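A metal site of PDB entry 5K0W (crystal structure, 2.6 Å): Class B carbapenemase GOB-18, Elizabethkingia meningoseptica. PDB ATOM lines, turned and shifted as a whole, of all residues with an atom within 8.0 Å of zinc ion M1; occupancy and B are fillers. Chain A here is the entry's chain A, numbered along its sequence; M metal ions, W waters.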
ATOM      1  N   TRP A  31      26.139  12.356 -23.748  1.00  0.00           N
ATOM      2  CA  TRP A  31      25.225  12.300 -24.885  1.00  0.00           C
ATOM      3  C   TRP A  31      25.711  11.443 -26.035  1.00  0.00           C
ATOM      4  O   TRP A  31      24.904  10.755 -26.672  1.00  0.00           O
ATOM      5  CB  TRP A  31      24.875  13.712 -25.367  1.00  0.00           C
ATOM      6  CG  TRP A  31      23.874  14.422 -24.504  1.00  0.00           C
ATOM      7  CD1 TRP A  31      23.520  14.122 -23.214  1.00  0.00           C
ATOM      8  CD2 TRP A  31      23.126  15.584 -24.869  1.00  0.00           C
ATOM      9  NE1 TRP A  31      22.600  15.026 -22.754  1.00  0.00           N
ATOM     10  CE2 TRP A  31      22.349  15.943 -23.742  1.00  0.00           C
ATOM     11  CE3 TRP A  31      23.066  16.384 -26.021  1.00  0.00           C
ATOM     12  CZ2 TRP A  31      21.484  17.048 -23.746  1.00  0.00           C
ATOM     13  CZ3 TRP A  31      22.224  17.484 -26.021  1.00  0.00           C
ATOM     14  CH2 TRP A  31      21.422  17.797 -24.907  1.00  0.00           C
ATOM     15  N   ASP A  51      23.410   8.741 -22.074  1.00  0.00           N
ATOM     16  CA  ASP A  51      22.290   9.546 -21.579  1.00  0.00           C
ATOM     17  C   ASP A  51      21.102   9.647 -22.537  1.00  0.00           C
ATOM     18  O   ASP A  51      19.969   9.805 -22.084  1.00  0.00           O
ATOM     19  CB  ASP A  51      22.739  10.949 -21.136  1.00  0.00           C
ATOM     20  CG  ASP A  51      21.680  11.653 -20.312  1.00  0.00           C
ATOM     21  OD1 ASP A  51      21.056  11.000 -19.438  1.00  0.00           O
ATOM     22  OD2 ASP A  51      21.453  12.850 -20.544  1.00  0.00           O
ATOM     23  N   LEU A  52      21.339   9.567 -23.856  1.00  0.00           N
ATOM     24  CA  LEU A  52      20.265   9.708 -24.824  1.00  0.00           C
ATOM     25  C   LEU A  52      19.560   8.418 -25.105  1.00  0.00           C
ATOM     26  O   LEU A  52      20.037   7.595 -25.900  1.00  0.00           O
ATOM     27  CB  LEU A  52      20.700  10.467 -26.094  1.00  0.00           C
ATOM     28  CG  LEU A  52      21.415  11.798 -25.841  1.00  0.00           C
ATOM     29  CD1 LEU A  52      21.930  12.413 -27.133  1.00  0.00           C
ATOM     30  CD2 LEU A  52      20.518  12.770 -25.094  1.00  0.00           C
ATOM     31  N   ALA A  53      18.422   8.230 -24.431  1.00  0.00           N
ATOM     32  CA  ALA A  53      17.615   7.024 -24.541  1.00  0.00           C
ATOM     33  C   ALA A  53      17.005   6.824 -25.924  1.00  0.00           C
ATOM     34  O   ALA A  53      16.403   7.750 -26.487  1.00  0.00           O
ATOM     35  CB  ALA A  53      16.525   7.025 -23.479  1.00  0.00           C
ATOM     36  N   ASN A  67      13.050   7.348 -30.556  1.00  0.00           N
ATOM     37  CA  ASN A  67      14.196   8.249 -30.313  1.00  0.00           C
ATOM     38  C   ASN A  67      15.554   7.815 -30.886  1.00  0.00           C
ATOM     39  O   ASN A  67      15.808   6.607 -30.955  1.00  0.00           O
ATOM     40  CB  ASN A  67      14.303   8.743 -28.863  1.00  0.00           C
ATOM     41  CG  ASN A  67      13.051   9.409 -28.362  1.00  0.00           C
ATOM     42  OD1 ASN A  67      12.141   9.796 -29.121  1.00  0.00           O
ATOM     43  ND2 ASN A  67      12.960   9.539 -27.061  1.00  0.00           N
ATOM     44  N   THR A  97       9.678  11.241 -28.912  1.00  0.00           N
ATOM     45  CA  THR A  97       9.053  11.739 -27.676  1.00  0.00           C
ATOM     46  C   THR A  97       9.102  13.277 -27.619  1.00  0.00           C
ATOM     47  O   THR A  97       8.346  13.870 -26.859  1.00  0.00           O
ATOM     48  CB  THR A  97       9.621  11.081 -26.412  1.00  0.00           C
ATOM     49  OG1 THR A  97      11.020  11.304 -26.342  1.00  0.00           O
ATOM     50  CG2 THR A  97       9.296   9.591 -26.326  1.00  0.00           C
ATOM     51  N   GLN A  98      10.014  13.899 -28.410  1.00  0.00           N
ATOM     52  CA  GLN A  98      10.221  15.338 -28.495  1.00  0.00           C
ATOM     53  C   GLN A  98      11.086  15.678 -29.729  1.00  0.00           C
ATOM     54  O   GLN A  98      11.990  14.913 -30.073  1.00  0.00           O
ATOM     55  CB  GLN A  98      10.876  15.895 -27.197  1.00  0.00           C
ATOM     56  CG  GLN A  98      12.156  15.178 -26.777  1.00  0.00           C
ATOM     57  CD  GLN A  98      12.932  15.962 -25.749  1.00  0.00           C
ATOM     58  OE1 GLN A  98      13.619  16.941 -26.078  1.00  0.00           O
ATOM     59  NE2 GLN A  98      12.897  15.494 -24.493  1.00  0.00           N
ATOM     60  N   HIS A 100      13.705  17.643 -30.601  1.00  0.00           N
ATOM     61  CA  HIS A 100      14.985  18.284 -30.314  1.00  0.00           C
ATOM     62  C   HIS A 100      16.094  17.422 -30.899  1.00  0.00           C
ATOM     63  O   HIS A 100      15.963  16.192 -30.866  1.00  0.00           O
ATOM     64  CB  HIS A 100      15.170  18.480 -28.814  1.00  0.00           C
ATOM     65  CG  HIS A 100      14.412  19.628 -28.233  1.00  0.00           C
ATOM     66  ND1 HIS A 100      14.128  19.692 -26.891  1.00  0.00           N
ATOM     67  CD2 HIS A 100      13.910  20.726 -28.843  1.00  0.00           C
ATOM     68  CE1 HIS A 100      13.460  20.819 -26.728  1.00  0.00           C
ATOM     69  NE2 HIS A 100      13.326  21.481 -27.864  1.00  0.00           N
ATOM     70  N   TYR A 101      17.161  18.048 -31.442  1.00  0.00           N
ATOM     71  CA  TYR A 101      18.333  17.392 -32.078  1.00  0.00           C
ATOM     72  C   TYR A 101      18.911  16.190 -31.293  1.00  0.00           C
ATOM     73  O   TYR A 101      19.428  15.266 -31.917  1.00  0.00           O
ATOM     74  CB  TYR A 101      19.439  18.410 -32.446  1.00  0.00           C
ATOM     75  CG  TYR A 101      20.297  18.835 -31.280  1.00  0.00           C
ATOM     76  CD1 TYR A 101      19.860  19.804 -30.387  1.00  0.00           C
ATOM     77  CD2 TYR A 101      21.558  18.277 -31.072  1.00  0.00           C
ATOM     78  CE1 TYR A 101      20.639  20.184 -29.296  1.00  0.00           C
ATOM     79  CE2 TYR A 101      22.354  18.673 -29.986  1.00  0.00           C
ATOM     80  CZ  TYR A 101      21.878  19.622 -29.094  1.00  0.00           C
ATOM     81  OH  TYR A 101      22.645  20.017 -28.035  1.00  0.00           O
ATOM     82  N   ASP A 102      18.830  16.230 -29.953  1.00  0.00           N
ATOM     83  CA  ASP A 102      19.340  15.164 -29.098  1.00  0.00           C
ATOM     84  C   ASP A 102      18.435  13.905 -29.080  1.00  0.00           C
ATOM     85  O   ASP A 102      18.762  12.928 -28.400  1.00  0.00           O
ATOM     86  CB  ASP A 102      19.675  15.678 -27.679  1.00  0.00           C
ATOM     87  CG  ASP A 102      18.518  16.268 -26.919  1.00  0.00           C
ATOM     88  OD1 ASP A 102      17.784  17.111 -27.495  1.00  0.00           O
ATOM     89  OD2 ASP A 102      18.377  15.951 -25.703  1.00  0.00           O
ATOM     90  N   HIS A 103      17.333  13.899 -29.842  1.00  0.00           N
ATOM     91  CA  HIS A 103      16.446  12.737 -30.002  1.00  0.00           C
ATOM     92  C   HIS A 103      16.088  12.537 -31.486  1.00  0.00           C
ATOM     93  O   HIS A 103      15.552  11.485 -31.851  1.00  0.00           O
ATOM     94  CB  HIS A 103      15.163  12.864 -29.150  1.00  0.00           C
ATOM     95  CG  HIS A 103      15.418  13.262 -27.725  1.00  0.00           C
ATOM     96  ND1 HIS A 103      15.712  12.317 -26.754  1.00  0.00           N
ATOM     97  CD2 HIS A 103      15.464  14.487 -27.165  1.00  0.00           C
ATOM     98  CE1 HIS A 103      15.910  13.003 -25.642  1.00  0.00           C
ATOM     99  NE2 HIS A 103      15.759  14.307 -25.845  1.00  0.00           N
ATOM    100  N   HIS A 175       7.521  20.841 -23.352  1.00  0.00           N
ATOM    101  CA  HIS A 175       8.936  20.745 -23.631  1.00  0.00           C
ATOM    102  C   HIS A 175       9.195  21.105 -25.102  1.00  0.00           C
ATOM    103  O   HIS A 175      10.148  21.812 -25.431  1.00  0.00           O
ATOM    104  CB  HIS A 175       9.471  19.366 -23.239  1.00  0.00           C
ATOM    105  CG  HIS A 175      10.961  19.265 -23.315  1.00  0.00           C
ATOM    106  ND1 HIS A 175      11.770  19.614 -22.240  1.00  0.00           N
ATOM    107  CD2 HIS A 175      11.746  18.890 -24.359  1.00  0.00           C
ATOM    108  CE1 HIS A 175      13.017  19.412 -22.654  1.00  0.00           C
ATOM    109  NE2 HIS A 175      13.055  18.978 -23.925  1.00  0.00           N
ATOM    110  N   ASN A 199       8.045  11.522 -21.568  1.00  0.00           N
ATOM    111  CA  ASN A 199       8.805  12.699 -21.901  1.00  0.00           C
ATOM    112  C   ASN A 199       8.499  13.677 -20.765  1.00  0.00           C
ATOM    113  O   ASN A 199       7.440  14.310 -20.752  1.00  0.00           O
ATOM    114  CB  ASN A 199       8.479  13.275 -23.283  1.00  0.00           C
ATOM    115  CG  ASN A 199       9.501  14.302 -23.692  1.00  0.00           C
ATOM    116  OD1 ASN A 199      10.620  13.974 -24.105  1.00  0.00           O
ATOM    117  ND2 ASN A 199       9.215  15.552 -23.423  1.00  0.00           N
ATOM    118  N   SER A 202       9.842  19.212 -18.402  1.00  0.00           N
ATOM    119  CA  SER A 202      10.779  20.247 -17.946  1.00  0.00           C
ATOM    120  C   SER A 202      10.626  21.551 -18.764  1.00  0.00           C
ATOM    121  O   SER A 202      10.092  21.528 -19.864  1.00  0.00           O
ATOM    122  CB  SER A 202      12.224  19.728 -17.993  1.00  0.00           C
ATOM    123  OG  SER A 202      12.475  18.988 -19.171  1.00  0.00           O
ATOM    124  N   ILE A 204      12.518  24.668 -20.643  1.00  0.00           N
ATOM    125  CA  ILE A 204      13.768  25.073 -21.320  1.00  0.00           C
ATOM    126  C   ILE A 204      13.950  26.595 -21.516  1.00  0.00           C
ATOM    127  O   ILE A 204      15.063  27.051 -21.816  1.00  0.00           O
ATOM    128  CB  ILE A 204      14.024  24.267 -22.620  1.00  0.00           C
ATOM    129  CG1 ILE A 204      12.987  24.607 -23.731  1.00  0.00           C
ATOM    130  CG2 ILE A 204      14.034  22.760 -22.278  1.00  0.00           C
ATOM    131  CD1 ILE A 204      13.248  24.002 -25.078  1.00  0.00           C
ATOM    132  N   SER A 240      13.124  10.058 -21.831  1.00  0.00           N
ATOM    133  CA  SER A 240      13.976  10.524 -22.937  1.00  0.00           C
ATOM    134  C   SER A 240      15.481  10.545 -22.599  1.00  0.00           C
ATOM    135  O   SER A 240      16.335  10.381 -23.477  1.00  0.00           O
ATOM    136  CB  SER A 240      13.545  11.919 -23.386  1.00  0.00           C
ATOM    137  OG  SER A 240      12.254  11.935 -23.982  1.00  0.00           O
ATOM    138  N   HIS A 241      15.800  10.782 -21.328  1.00  0.00           N
ATOM    139  CA  HIS A 241      17.168  10.830 -20.791  1.00  0.00           C
ATOM    140  C   HIS A 241      17.349   9.804 -19.674  1.00  0.00           C
ATOM    141  O   HIS A 241      16.466   9.650 -18.821  1.00  0.00           O
ATOM    142  CB  HIS A 241      17.474  12.227 -20.293  1.00  0.00           C
ATOM    143  CG  HIS A 241      17.673  13.226 -21.385  1.00  0.00           C
ATOM    144  ND1 HIS A 241      18.946  13.610 -21.800  1.00  0.00           N
ATOM    145  CD2 HIS A 241      16.759  13.857 -22.153  1.00  0.00           C
ATOM    146  CE1 HIS A 241      18.759  14.478 -22.782  1.00  0.00           C
ATOM    147  NE2 HIS A 241      17.473  14.642 -23.045  1.00  0.00           N
ATOM    148  N   GLN A 244      16.953  10.749 -15.886  1.00  0.00           N
ATOM    149  CA  GLN A 244      15.579  10.996 -15.437  1.00  0.00           C
ATOM    150  C   GLN A 244      14.945   9.809 -14.734  1.00  0.00           C
ATOM    151  O   GLN A 244      14.168   9.998 -13.792  1.00  0.00           O
ATOM    152  CB  GLN A 244      14.702  11.479 -16.585  1.00  0.00           C
ATOM    153  CG  GLN A 244      15.104  12.865 -17.068  1.00  0.00           C
ATOM    154  CD  GLN A 244      14.416  13.273 -18.335  1.00  0.00           C
ATOM    155  OE1 GLN A 244      14.238  12.479 -19.268  1.00  0.00           O
ATOM    156  NE2 GLN A 244      14.037  14.518 -18.428  1.00  0.00           N
HETATM  157 ZN    ZN M   1      16.611  15.751 -24.576  1.00  0.00          ZN
HETATM  158 ZN    ZN M   2      14.568  18.537 -25.244  1.00  0.00          ZN
HETATM  159  O   HOH W   1      15.642  17.429 -23.862  1.00  0.00           O
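OE1 of Gln 244 is in hydrogen-bond range of N of His 241 (3.1 Å).
OD2 of Asp 51 lies within hydrogen-bond range of ND1 of His 241, at 2.9 Å.
NE2 of His 103 sits close to NE2 of Gln 98 (3.4 Å).
The side-chain amide nitrogen of Gln 98 lies within hydrogen-bond range of the side-chain amide oxygen of Asn 199 (2.8 Å).
Zinc ion M1 is bound by water W1, a ring nitrogen (NE2) of His 241, a ring nitrogen (NE2) of His 103 and the side-chain carboxylate (OD2) of Asp 102.
Zinc ion M1 has four donor atoms within binding distance.
Gln 98 touches zinc ion M1 (OE1 to ZN, 3.6 Å).
Of the 18 residues printed, 4 come within 4 Å of zinc ion M1.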
